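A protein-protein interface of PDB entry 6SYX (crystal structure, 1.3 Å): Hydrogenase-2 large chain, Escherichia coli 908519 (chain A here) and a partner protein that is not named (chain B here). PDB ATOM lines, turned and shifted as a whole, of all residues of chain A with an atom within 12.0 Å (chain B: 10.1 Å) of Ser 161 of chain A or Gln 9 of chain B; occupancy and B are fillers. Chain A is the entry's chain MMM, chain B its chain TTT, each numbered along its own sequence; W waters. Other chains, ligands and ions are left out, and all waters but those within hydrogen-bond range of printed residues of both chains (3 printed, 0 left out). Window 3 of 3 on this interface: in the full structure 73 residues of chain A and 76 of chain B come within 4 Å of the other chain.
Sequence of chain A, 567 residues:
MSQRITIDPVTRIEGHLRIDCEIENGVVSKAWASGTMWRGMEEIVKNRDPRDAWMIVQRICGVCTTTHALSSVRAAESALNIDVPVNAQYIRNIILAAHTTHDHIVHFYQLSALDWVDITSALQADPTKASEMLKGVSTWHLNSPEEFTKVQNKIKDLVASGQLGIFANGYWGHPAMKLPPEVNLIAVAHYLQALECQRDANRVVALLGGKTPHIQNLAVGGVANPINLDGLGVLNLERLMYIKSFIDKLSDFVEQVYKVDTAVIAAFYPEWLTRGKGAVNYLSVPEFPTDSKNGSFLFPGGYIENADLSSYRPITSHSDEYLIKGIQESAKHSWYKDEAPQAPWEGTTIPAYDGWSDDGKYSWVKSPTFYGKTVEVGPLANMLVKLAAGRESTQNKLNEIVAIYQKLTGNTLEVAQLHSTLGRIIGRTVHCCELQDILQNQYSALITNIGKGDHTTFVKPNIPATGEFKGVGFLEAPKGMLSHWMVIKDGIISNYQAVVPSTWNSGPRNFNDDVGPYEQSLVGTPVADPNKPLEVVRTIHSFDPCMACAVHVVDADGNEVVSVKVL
The backbone carbonyl oxygen (O) of Leu 46 of chain B is in hydrogen-bond range of the backbone NH (N) of Ile 166 of chain A (3.0 Å).
NH2 of Arg 10 of chain B is in hydrogen-bond range of OG of Ser 161 of chain A (3.2 Å).
NE2 of Gln 9 of chain B sits at hydrogen-bond distance from O of Ser 161 of chain A (2.9 Å).
OE1 of Gln 163 of chain A sits close to OE1 of Gln 9 of chain B (3.5 Å).
The side-chain hydroxyl of Tyr 71 of chain B is in hydrogen-bond range of the side-chain amide nitrogen of Gln 163 of chain A, at 3.1 Å.
N of Arg 10 of chain B sits at hydrogen-bond distance from OE1 of Gln 163 of chain A, 2.8 Å away.
Leu 158 of chain A touches Arg 10 of chain B.
Gln 163 of chain A touches Ser 45 of chain B (NE2 to CB, 3.7 Å).
Gly 165 of chain A touches Leu 46 of chain B.
Gly 165 of chain A touches Glu 47 of chain B (CA to OE1, 3.9 Å).
Of the printed residues of chain B, Leu 158 of chain A touches Arg 10 (3.7 Å).
Val 159 of chain A touches none of the printed residues of chain B.
No residue of chain B comes within 4 Å of Ala 160 of chain A.
Ser 161 of chain A touches just these residues of chain B: Gln 9 and Arg 10.
No residue of chain B comes within 4 Å of Gly 162 of chain A.
Of the printed residues of chain B, Ile 166 of chain A touches Leu 46 (3.0 Å).
Phe 167 of chain A touches none of the printed residues of chain B.
No residue of chain A comes within 4 Å of Pro 8 of chain B.
Printed residues of chain A within 4 Å of Gln 9 of chain B: Ser 161 (2.9 Å) and Gln 163 (3.3 Å).
Printed residues of chain A within 4 Å of Arg 10 of chain B: Leu 158 (3.7 Å), Ser 161 (3.2 Å) and Gln 163 (2.8 Å).
No residue of chain A comes within 4 Å of Pro 11 of chain B.
Of the printed residues of chain A, Ser 45 of chain B touches Gln 163.
Water W1 lies within hydrogen-bond range of the side-chain amide oxygen of Gln 163 of chain A, the backbone carbonyl oxygen of Pro 8 of chain B, the guanidinium group of Arg 10 of chain B and the side-chain hydroxyl of Ser 161 of chain A.
Water W2 lies within hydrogen-bond range of O of Gln 163 of chain A (2.8 Å), OG of Ser 45 of chain B (2.9 Å) and NH1 of Arg 10 of chain B (3.0 Å).
Water W3 bridges the side-chain carboxylate of Glu 42 of chain B and the side-chain amino group of Lys 154 of chain A.
OG of Ser 45 of chain B is in hydrogen-bond range of OE2 of Glu 47 of chain B, 2.6 Å away.
OE2 of Glu 47 of chain B sits at hydrogen-bond distance from OH of Tyr 71 of chain B, at 3.2 Å.
O of Pro 11 of chain B lies within hydrogen-bond range of N of Ser 45 of chain B, 2.9 Å away.
NZ of Lys 70 of chain B lies within hydrogen-bond range of OH of Tyr 71 of chain B (3.4 Å).
OG of Ser 161 of chain A sits close to N of Gln 163 of chain A, at 3.2 Å.
O of Val 40 of chain B sits at hydrogen-bond distance from NH1 of Arg 10 of chain B.
Of the 19 printed residues of chain A, 5 touch a printed residue of chain B.
Printed residues of chain A that touch a printed residue of chain B: Leu 158, Ser 161, Gln 163, Gly 165 and Ile 166.
Along chain A the printed residues that touch a printed residue of chain B span positions 158 to 166.
Of the 17 printed residues of chain B, 6 touch a printed residue of chain A.
Hydrophobic or aromatic side chains of chain B that line the printed part of chain A: Tyr 71.
Among the printed residues, 10 pairs touch across the chains.
Among the printed residues, no Asp or Glu carboxylate lies within 4 Å of a Lys or Arg side-chain nitrogen of the other chain.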
ATOM      1  N   ILE A 119      -6.587  21.798  -4.985  1.00  0.00           N
ATOM      2  CA  ILE A 119      -5.609  20.927  -4.262  1.00  0.00           C
ATOM      3  C   ILE A 119      -6.252  20.291  -3.014  1.00  0.00           C
ATOM      4  O   ILE A 119      -5.825  19.171  -2.688  1.00  0.00           O
ATOM      5  CB  ILE A 119      -4.268  21.606  -3.923  1.00  0.00           C
ATOM      6  CG1 ILE A 119      -4.389  22.654  -2.811  1.00  0.00           C
ATOM      7  CG2 ILE A 119      -3.599  22.142  -5.186  1.00  0.00           C
ATOM      8  CD1 ILE A 119      -3.083  22.898  -2.042  1.00  0.00           C
ATOM      9  N   LEU A 123      -7.054  15.696  -1.390  1.00  0.00           N
ATOM     10  CA  LEU A 123      -6.983  14.941  -0.103  1.00  0.00           C
ATOM     11  C   LEU A 123      -8.067  13.875  -0.009  1.00  0.00           C
ATOM     12  O   LEU A 123      -7.872  12.918   0.767  1.00  0.00           O
ATOM     13  CB  LEU A 123      -7.114  15.878   1.095  1.00  0.00           C
ATOM     14  CG  LEU A 123      -5.985  16.884   1.270  1.00  0.00           C
ATOM     15  CD1 LEU A 123      -6.354  17.917   2.320  1.00  0.00           C
ATOM     16  CD2 LEU A 123      -4.673  16.185   1.598  1.00  0.00           C
ATOM     17  N   GLN A 152       0.109  12.791  -2.272  1.00  0.00           N
ATOM     18  CA  GLN A 152      -1.033  13.092  -1.332  1.00  0.00           C
ATOM     19  C   GLN A 152      -0.508  13.381   0.078  1.00  0.00           C
ATOM     20  O   GLN A 152      -1.019  14.308   0.727  1.00  0.00           O
ATOM     21  CB  GLN A 152      -2.066  11.953  -1.362  1.00  0.00           C
ATOM     22  CG  GLN A 152      -3.388  12.261  -0.624  1.00  0.00           C
ATOM     23  CD  GLN A 152      -4.392  11.126  -0.719  1.00  0.00           C
ATOM     24  OE1 GLN A 152      -4.103   9.981  -0.332  1.00  0.00           O
ATOM     25  NE2 GLN A 152      -5.548  11.433  -1.323  1.00  0.00           N
ATOM     26  N   ASN A 153       0.491  12.623   0.549  1.00  0.00           N
ATOM     27  CA  ASN A 153       1.099  12.845   1.900  1.00  0.00           C
ATOM     28  C   ASN A 153       1.854  14.184   1.964  1.00  0.00           C
ATOM     29  O   ASN A 153       1.817  14.859   3.002  1.00  0.00           O
ATOM     30  CB  ASN A 153       1.971  11.664   2.341  1.00  0.00           C
ATOM     31  CG  ASN A 153       1.177  10.406   2.644  1.00  0.00           C
ATOM     32  OD1 ASN A 153      -0.031  10.474   2.843  1.00  0.00           O
ATOM     33  ND2 ASN A 153       1.851   9.275   2.663  1.00  0.00           N
ATOM     34  N   LYS A 154       2.448  14.650   0.862  1.00  0.00           N
ATOM     35  CA  LYS A 154       3.079  15.995   0.880  1.00  0.00           C
ATOM     36  C   LYS A 154       1.978  17.061   1.041  1.00  0.00           C
ATOM     37  O   LYS A 154       2.213  18.012   1.781  1.00  0.00           O
ATOM     38  CB  LYS A 154       3.909  16.267  -0.387  1.00  0.00           C
ATOM     39  CG  LYS A 154       5.186  15.453  -0.543  1.00  0.00           C
ATOM     40  CD  LYS A 154       5.822  15.701  -1.910  1.00  0.00           C
ATOM     41  CE  LYS A 154       6.880  14.681  -2.257  1.00  0.00           C
ATOM     42  NZ  LYS A 154       8.226  15.150  -1.862  1.00  0.00           N
ATOM     43  N   ILE A 155       0.842  16.922   0.352  1.00  0.00           N
ATOM     44  CA  ILE A 155      -0.283  17.904   0.480  1.00  0.00           C
ATOM     45  C   ILE A 155      -0.787  17.881   1.945  1.00  0.00           C
ATOM     46  O   ILE A 155      -0.993  18.965   2.551  1.00  0.00           O
ATOM     47  CB  ILE A 155      -1.448  17.607  -0.485  1.00  0.00           C
ATOM     48  CG1 ILE A 155      -0.980  17.547  -1.940  1.00  0.00           C
ATOM     49  CG2 ILE A 155      -2.577  18.637  -0.302  1.00  0.00           C
ATOM     50  CD1 ILE A 155      -2.062  17.036  -2.889  1.00  0.00           C
ATOM     51  N   LYS A 156      -0.979  16.677   2.465  1.00  0.00           N
ATOM     52  CA  LYS A 156      -1.520  16.463   3.845  1.00  0.00           C
ATOM     53  C   LYS A 156      -0.609  17.167   4.854  1.00  0.00           C
ATOM     54  O   LYS A 156      -1.138  17.889   5.764  1.00  0.00           O
ATOM     55  CB  LYS A 156      -1.697  14.962   4.078  1.00  0.00           C
ATOM     56  CG  LYS A 156      -2.307  14.544   5.398  1.00  0.00           C
ATOM     57  CD  LYS A 156      -2.532  13.024   5.509  1.00  0.00           C
ATOM     58  CE  LYS A 156      -2.965  12.360   4.214  1.00  0.00           C
ATOM     59  NZ  LYS A 156      -3.853  11.194   4.456  1.00  0.00           N
ATOM     60  N   ASP A 157       0.714  17.033   4.699  1.00  0.00           N
ATOM     61  CA  ASP A 157       1.700  17.663   5.618  1.00  0.00           C
ATOM     62  C   ASP A 157       1.650  19.193   5.507  1.00  0.00           C
ATOM     63  O   ASP A 157       1.815  19.889   6.551  1.00  0.00           O
ATOM     64  CB  ASP A 157       3.123  17.153   5.358  1.00  0.00           C
ATOM     65  CG  ASP A 157       3.360  15.698   5.716  1.00  0.00           C
ATOM     66  OD1 ASP A 157       2.545  15.143   6.480  1.00  0.00           O
ATOM     67  OD2 ASP A 157       4.377  15.147   5.244  1.00  0.00           O
ATOM     68  N   LEU A 158       1.553  19.754   4.289  1.00  0.00           N
ATOM     69  CA  LEU A 158       1.497  21.219   4.088  1.00  0.00           C
ATOM     70  C   LEU A 158       0.256  21.753   4.821  1.00  0.00           C
ATOM     71  O   LEU A 158       0.401  22.752   5.592  1.00  0.00           O
ATOM     72  CB  LEU A 158       1.462  21.516   2.580  1.00  0.00           C
ATOM     73  CG  LEU A 158       1.381  23.003   2.203  1.00  0.00           C
ATOM     74  CD1 LEU A 158       2.710  23.668   2.398  1.00  0.00           C
ATOM     75  CD2 LEU A 158       0.932  23.198   0.750  1.00  0.00           C
ATOM     76  N   VAL A 159      -0.890  21.103   4.614  1.00  0.00           N
ATOM     77  CA  VAL A 159      -2.182  21.574   5.199  1.00  0.00           C
ATOM     78  C   VAL A 159      -2.084  21.463   6.726  1.00  0.00           C
ATOM     79  O   VAL A 159      -2.429  22.465   7.432  1.00  0.00           O
ATOM     80  CB  VAL A 159      -3.381  20.806   4.613  1.00  0.00           C
ATOM     81  CG1 VAL A 159      -4.649  21.094   5.408  1.00  0.00           C
ATOM     82  CG2 VAL A 159      -3.601  21.144   3.159  1.00  0.00           C
ATOM     83  N   ALA A 160      -1.541  20.360   7.230  1.00  0.00           N
ATOM     84  CA  ALA A 160      -1.430  20.098   8.686  1.00  0.00           C
ATOM     85  C   ALA A 160      -0.537  21.153   9.360  1.00  0.00           C
ATOM     86  O   ALA A 160      -0.752  21.428  10.559  1.00  0.00           O
ATOM     87  CB  ALA A 160      -0.942  18.694   8.932  1.00  0.00           C
ATOM     88  N   SER A 161       0.429  21.770   8.662  1.00  0.00           N
ATOM     89  CA  SER A 161       1.324  22.803   9.249  1.00  0.00           C
ATOM     90  C   SER A 161       0.583  24.125   9.499  1.00  0.00           C
ATOM     91  O   SER A 161       1.125  24.908  10.260  1.00  0.00           O
ATOM     92  CB  SER A 161       2.549  23.056   8.371  1.00  0.00           C
ATOM     93  OG  SER A 161       2.198  23.847   7.212  1.00  0.00           O
ATOM     94  N   GLY A 162      -0.574  24.381   8.896  1.00  0.00           N
ATOM     95  CA  GLY A 162      -1.279  25.675   8.976  1.00  0.00           C
ATOM     96  C   GLY A 162      -0.568  26.799   8.214  1.00  0.00           C
ATOM     97  O   GLY A 162      -0.976  27.957   8.355  1.00  0.00           O
ATOM     98  N   GLN A 163       0.483  26.499   7.428  1.00  0.00           N
ATOM     99  CA  GLN A 163       1.235  27.512   6.632  1.00  0.00           C
ATOM    100  C   GLN A 163       1.059  27.153   5.151  1.00  0.00           C
ATOM    101  O   GLN A 163       1.934  26.423   4.579  1.00  0.00           O
ATOM    102  CB  GLN A 163       2.727  27.567   6.991  1.00  0.00           C
ATOM    103  CG  GLN A 163       3.090  28.054   8.392  1.00  0.00           C
ATOM    104  CD  GLN A 163       4.582  28.090   8.619  1.00  0.00           C
ATOM    105  OE1 GLN A 163       5.225  27.039   8.645  1.00  0.00           O
ATOM    106  NE2 GLN A 163       5.124  29.304   8.667  1.00  0.00           N
ATOM    107  N   LEU A 164      -0.049  27.562   4.537  1.00  0.00           N
ATOM    108  CA  LEU A 164      -0.298  27.190   3.114  1.00  0.00           C
ATOM    109  C   LEU A 164       0.486  28.132   2.160  1.00  0.00           C
ATOM    110  O   LEU A 164       0.712  27.716   0.997  1.00  0.00           O
ATOM    111  CB  LEU A 164      -1.806  27.261   2.841  1.00  0.00           C
ATOM    112  CG  LEU A 164      -2.693  26.420   3.762  1.00  0.00           C
ATOM    113  CD1 LEU A 164      -4.182  26.778   3.580  1.00  0.00           C
ATOM    114  CD2 LEU A 164      -2.453  24.970   3.486  1.00  0.00           C
ATOM    115  N   GLY A 165       0.878  29.305   2.617  1.00  0.00           N
ATOM    116  CA  GLY A 165       1.657  30.300   1.844  1.00  0.00           C
ATOM    117  C   GLY A 165       1.043  30.581   0.476  1.00  0.00           C
ATOM    118  O   GLY A 165      -0.132  30.912   0.384  1.00  0.00           O
ATOM    119  N   ILE A 166       1.788  30.357  -0.575  1.00  0.00           N
ATOM    120  CA  ILE A 166       1.321  30.648  -1.970  1.00  0.00           C
ATOM    121  C   ILE A 166       0.165  29.721  -2.388  1.00  0.00           C
ATOM    122  O   ILE A 166      -0.516  30.037  -3.377  1.00  0.00           O
ATOM    123  CB  ILE A 166       2.492  30.577  -2.965  1.00  0.00           C
ATOM    124  CG1 ILE A 166       3.296  29.288  -2.821  1.00  0.00           C
ATOM    125  CG2 ILE A 166       3.365  31.829  -2.842  1.00  0.00           C
ATOM    126  CD1 ILE A 166       4.297  29.059  -3.920  1.00  0.00           C
ATOM    127  N   PHE A 167      -0.104  28.613  -1.691  1.00  0.00           N
ATOM    128  CA  PHE A 167      -1.287  27.761  -1.968  1.00  0.00           C
ATOM    129  C   PHE A 167      -2.547  28.248  -1.187  1.00  0.00           C
ATOM    130  O   PHE A 167      -3.622  27.671  -1.435  1.00  0.00           O
ATOM    131  CB  PHE A 167      -0.886  26.288  -1.789  1.00  0.00           C
ATOM    132  CG  PHE A 167       0.323  25.886  -2.587  1.00  0.00           C
ATOM    133  CD1 PHE A 167       0.236  25.711  -3.962  1.00  0.00           C
ATOM    134  CD2 PHE A 167       1.567  25.770  -1.985  1.00  0.00           C
ATOM    135  CE1 PHE A 167       1.360  25.367  -4.694  1.00  0.00           C
ATOM    136  CE2 PHE A 167       2.690  25.427  -2.719  1.00  0.00           C
ATOM    137  CZ  PHE A 167       2.587  25.242  -4.083  1.00  0.00           C
ATOM    138  N   ALA A 168      -2.488  29.283  -0.349  1.00  0.00           N
ATOM    139  CA  ALA A 168      -3.615  29.760   0.521  1.00  0.00           C
ATOM    140  C   ALA A 168      -4.664  30.630  -0.187  1.00  0.00           C
ATOM    141  O   ALA A 168      -4.337  31.262  -1.231  1.00  0.00           O
ATOM    142  CB  ALA A 168      -3.094  30.608   1.622  1.00  0.00           C
ATOM    143  N   PRO B   8       5.999  20.933  11.696  1.00  0.00           N
ATOM    144  CA  PRO B   8       7.090  21.867  12.109  1.00  0.00           C
ATOM    145  C   PRO B   8       7.061  23.186  11.296  1.00  0.00           C
ATOM    146  O   PRO B   8       7.058  23.107  10.067  1.00  0.00           O
ATOM    147  CB  PRO B   8       8.394  21.075  11.880  1.00  0.00           C
ATOM    148  CG  PRO B   8       8.040  20.069  10.790  1.00  0.00           C
ATOM    149  CD  PRO B   8       6.564  19.764  10.986  1.00  0.00           C
ATOM    150  N   GLN B   9       7.033  24.353  11.966  1.00  0.00           N
ATOM    151  CA  GLN B   9       6.846  25.684  11.301  1.00  0.00           C
ATOM    152  C   GLN B   9       8.087  26.089  10.494  1.00  0.00           C
ATOM    153  O   GLN B   9       9.221  25.859  10.941  1.00  0.00           O
ATOM    154  CB  GLN B   9       6.519  26.796  12.297  1.00  0.00           C
ATOM    155  CG  GLN B   9       5.200  26.542  13.041  1.00  0.00           C
ATOM    156  CD  GLN B   9       3.990  26.409  12.138  1.00  0.00           C
ATOM    157  OE1 GLN B   9       3.458  27.387  11.627  1.00  0.00           O
ATOM    158  NE2 GLN B   9       3.518  25.183  11.944  1.00  0.00           N
ATOM    159  N   ARG B  10       7.876  26.681   9.318  1.00  0.00           N
ATOM    160  CA  ARG B  10       8.978  27.099   8.415  1.00  0.00           C
ATOM    161  C   ARG B  10       9.128  28.611   8.452  1.00  0.00           C
ATOM    162  O   ARG B  10       8.138  29.357   8.613  1.00  0.00           O
ATOM    163  CB  ARG B  10       8.647  26.620   6.993  1.00  0.00           C
ATOM    164  CG  ARG B  10       8.818  25.118   6.818  1.00  0.00           C
ATOM    165  CD  ARG B  10       8.205  24.545   5.547  1.00  0.00           C
ATOM    166  NE  ARG B  10       6.759  24.487   5.732  1.00  0.00           N
ATOM    167  CZ  ARG B  10       5.829  25.089   5.002  1.00  0.00           C
ATOM    168  NH1 ARG B  10       6.127  25.731   3.883  1.00  0.00           N
ATOM    169  NH2 ARG B  10       4.550  24.899   5.311  1.00  0.00           N
ATOM    170  N   PRO B  11      10.341  29.135   8.271  1.00  0.00           N
ATOM    171  CA  PRO B  11      10.581  30.571   8.304  1.00  0.00           C
ATOM    172  C   PRO B  11       9.867  31.311   7.159  1.00  0.00           C
ATOM    173  O   PRO B  11       9.972  30.939   5.972  1.00  0.00           O
ATOM    174  CB  PRO B  11      12.092  30.788   8.187  1.00  0.00           C
ATOM    175  CG  PRO B  11      12.670  29.407   7.945  1.00  0.00           C
ATOM    176  CD  PRO B  11      11.602  28.370   8.162  1.00  0.00           C
ATOM    177  N   PRO B  12       9.136  32.407   7.467  1.00  0.00           N
ATOM    178  CA  PRO B  12       8.339  33.105   6.453  1.00  0.00           C
ATOM    179  C   PRO B  12       9.171  34.070   5.579  1.00  0.00           C
ATOM    180  O   PRO B  12      10.155  34.700   6.030  1.00  0.00           O
ATOM    181  CB  PRO B  12       7.289  33.860   7.274  1.00  0.00           C
ATOM    182  CG  PRO B  12       8.045  34.182   8.533  1.00  0.00           C
ATOM    183  CD  PRO B  12       8.884  32.947   8.825  1.00  0.00           C
ATOM    184  N   VAL B  40       9.977  25.580  -1.295  1.00  0.00           N
ATOM    185  CA  VAL B  40       8.637  26.113  -0.889  1.00  0.00           C
ATOM    186  C   VAL B  40       7.913  25.087  -0.007  1.00  0.00           C
ATOM    187  O   VAL B  40       7.023  25.556   0.754  1.00  0.00           O
ATOM    188  CB  VAL B  40       7.806  26.595  -2.088  1.00  0.00           C
ATOM    189  CG1 VAL B  40       8.540  27.699  -2.847  1.00  0.00           C
ATOM    190  CG2 VAL B  40       7.301  25.496  -2.951  1.00  0.00           C
ATOM    191  N   LEU B  41       8.263  23.809  -0.006  1.00  0.00           N
ATOM    192  CA  LEU B  41       7.549  22.775   0.820  1.00  0.00           C
ATOM    193  C   LEU B  41       8.315  22.497   2.123  1.00  0.00           C
ATOM    194  O   LEU B  41       7.660  22.131   3.123  1.00  0.00           O
ATOM    195  CB  LEU B  41       7.289  21.493   0.022  1.00  0.00           C
ATOM    196  CG  LEU B  41       6.332  21.654  -1.159  1.00  0.00           C
ATOM    197  CD1 LEU B  41       6.200  20.343  -1.905  1.00  0.00           C
ATOM    198  CD2 LEU B  41       4.959  22.169  -0.706  1.00  0.00           C
ATOM    199  N   GLU B  42       9.638  22.640   2.140  1.00  0.00           N
ATOM    200  CA  GLU B  42      10.505  22.183   3.264  1.00  0.00           C
ATOM    201  C   GLU B  42      11.325  23.318   3.872  1.00  0.00           C
ATOM    202  O   GLU B  42      11.415  23.377   5.128  1.00  0.00           O
ATOM    203  CB  GLU B  42      11.488  21.084   2.833  1.00  0.00           C
ATOM    204  CG  GLU B  42      10.867  19.956   2.069  1.00  0.00           C
ATOM    205  CD  GLU B  42      10.103  18.942   2.878  1.00  0.00           C
ATOM    206  OE1 GLU B  42      10.102  19.059   4.129  1.00  0.00           O
ATOM    207  OE2 GLU B  42       9.521  18.027   2.241  1.00  0.00           O
ATOM    208  N   THR B  43      11.960  24.193   3.121  1.00  0.00           N
ATOM    209  CA  THR B  43      12.969  25.148   3.669  1.00  0.00           C
ATOM    210  C   THR B  43      12.295  26.422   4.230  1.00  0.00           C
ATOM    211  O   THR B  43      12.731  26.914   5.340  1.00  0.00           O
ATOM    212  CB  THR B  43      14.002  25.559   2.618  1.00  0.00           C
ATOM    213  OG1 THR B  43      14.473  24.392   1.924  1.00  0.00           O
ATOM    214  CG2 THR B  43      15.163  26.334   3.198  1.00  0.00           C
ATOM    215  N   ILE B  44      11.349  27.015   3.482  1.00  0.00           N
ATOM    216  CA  ILE B  44      10.695  28.301   3.871  1.00  0.00           C
ATOM    217  C   ILE B  44       9.188  28.097   3.747  1.00  0.00           C
ATOM    218  O   ILE B  44       8.670  27.097   3.186  1.00  0.00           O
ATOM    219  CB  ILE B  44      11.183  29.504   3.001  1.00  0.00           C
ATOM    220  CG1 ILE B  44      10.812  29.338   1.512  1.00  0.00           C
ATOM    221  CG2 ILE B  44      12.676  29.717   3.202  1.00  0.00           C
ATOM    222  CD1 ILE B  44      11.003  30.555   0.616  1.00  0.00           C
ATOM    223  N   SER B  45       8.461  29.087   4.285  1.00  0.00           N
ATOM    224  CA  SER B  45       7.052  29.331   3.916  1.00  0.00           C
ATOM    225  C   SER B  45       7.030  30.597   3.053  1.00  0.00           C
ATOM    226  O   SER B  45       7.273  31.709   3.574  1.00  0.00           O
ATOM    227  CB  SER B  45       6.102  29.474   5.126  1.00  0.00           C
ATOM    228  OG  SER B  45       4.786  29.648   4.641  1.00  0.00           O
ATOM    229  N   LEU B  46       6.741  30.430   1.743  1.00  0.00           N
ATOM    230  CA  LEU B  46       6.679  31.553   0.785  1.00  0.00           C
ATOM    231  C   LEU B  46       5.281  32.157   0.944  1.00  0.00           C
ATOM    232  O   LEU B  46       4.335  31.603   0.396  1.00  0.00           O
ATOM    233  CB  LEU B  46       7.008  31.057  -0.628  1.00  0.00           C
ATOM    234  CG  LEU B  46       7.187  32.144  -1.690  1.00  0.00           C
ATOM    235  CD1 LEU B  46       8.173  33.222  -1.288  1.00  0.00           C
ATOM    236  CD2 LEU B  46       7.593  31.495  -3.027  1.00  0.00           C
ATOM    237  N   GLU B  47       5.185  33.246   1.708  1.00  0.00           N
ATOM    238  CA  GLU B  47       3.871  33.810   2.144  1.00  0.00           C
ATOM    239  C   GLU B  47       3.272  34.730   1.065  1.00  0.00           C
ATOM    240  O   GLU B  47       2.041  34.943   1.036  1.00  0.00           O
ATOM    241  CB  GLU B  47       4.039  34.547   3.477  1.00  0.00           C
ATOM    242  CG  GLU B  47       4.317  33.615   4.627  1.00  0.00           C
ATOM    243  CD  GLU B  47       3.171  32.680   5.004  1.00  0.00           C
ATOM    244  OE1 GLU B  47       1.975  32.984   4.712  1.00  0.00           O
ATOM    245  OE2 GLU B  47       3.480  31.677   5.674  1.00  0.00           O
ATOM    246  N   LYS B  70       0.759  38.736  11.042  1.00  0.00           N
ATOM    247  CA  LYS B  70       1.089  37.471  11.725  1.00  0.00           C
ATOM    248  C   LYS B  70       2.604  37.404  12.021  1.00  0.00           C
ATOM    249  O   LYS B  70       2.996  36.958  13.122  1.00  0.00           O
ATOM    250  CB  LYS B  70       0.551  36.279  10.932  1.00  0.00           C
ATOM    251  CG  LYS B  70       0.844  34.933  11.573  1.00  0.00           C
ATOM    252  CD  LYS B  70       0.202  33.782  10.859  1.00  0.00           C
ATOM    253  CE  LYS B  70       0.574  32.445  11.463  1.00  0.00           C
ATOM    254  NZ  LYS B  70       0.143  31.319  10.590  1.00  0.00           N
ATOM    255  N   TYR B  71       3.468  37.689  11.038  1.00  0.00           N
ATOM    256  CA  TYR B  71       4.907  37.384  11.132  1.00  0.00           C
ATOM    257  C   TYR B  71       5.702  38.663  11.348  1.00  0.00           C
ATOM    258  O   TYR B  71       6.926  38.669  11.110  1.00  0.00           O
ATOM    259  CB  TYR B  71       5.366  36.674   9.850  1.00  0.00           C
ATOM    260  CG  TYR B  71       4.706  35.344   9.612  1.00  0.00           C
ATOM    261  CD1 TYR B  71       4.932  34.256  10.452  1.00  0.00           C
ATOM    262  CD2 TYR B  71       3.867  35.145   8.536  1.00  0.00           C
ATOM    263  CE1 TYR B  71       4.362  33.022  10.199  1.00  0.00           C
ATOM    264  CE2 TYR B  71       3.281  33.920   8.279  1.00  0.00           C
ATOM    265  CZ  TYR B  71       3.537  32.842   9.114  1.00  0.00           C
ATOM    266  OH  TYR B  71       3.011  31.599   8.876  1.00  0.00           O
ATOM    267  N   GLN B  74       9.600  38.836  11.953  1.00  0.00           N
ATOM    268  CA  GLN B  74      10.132  37.467  11.711  1.00  0.00           C
ATOM    269  C   GLN B  74      10.474  37.190  10.239  1.00  0.00           C
ATOM    270  O   GLN B  74      11.285  36.281  10.010  1.00  0.00           O
ATOM    271  CB  GLN B  74       9.151  36.398  12.164  1.00  0.00           C
ATOM    272  CG  GLN B  74       8.859  36.489  13.665  1.00  0.00           C
ATOM    273  CD  GLN B  74       7.911  35.393  14.068  1.00  0.00           C
ATOM    274  OE1 GLN B  74       6.792  35.288  13.578  1.00  0.00           O
ATOM    275  NE2 GLN B  74       8.366  34.549  14.983  1.00  0.00           N
ATOM    276  N   ILE B 168      18.770  31.234   8.477  1.00  0.00           N
ATOM    277  CA  ILE B 168      17.928  30.213   9.166  1.00  0.00           C
ATOM    278  C   ILE B 168      18.819  29.379  10.118  1.00  0.00           C
ATOM    279  O   ILE B 168      18.382  29.093  11.274  1.00  0.00           O
ATOM    280  CB  ILE B 168      17.201  29.321   8.145  1.00  0.00           C
ATOM    281  CG1 ILE B 168      16.252  30.143   7.269  1.00  0.00           C
ATOM    282  CG2 ILE B 168      16.480  28.152   8.829  1.00  0.00           C
ATOM    283  CD1 ILE B 168      15.778  29.351   6.042  1.00  0.00           C
HETATM  284  O   HOH W   1       5.281  24.359   8.251  1.00  0.00           O
HETATM  285  O   HOH W   2       3.881  27.523   2.932  1.00  0.00           O
HETATM  286  O   HOH W   3       8.828  18.014  -0.739  1.00  0.00           O
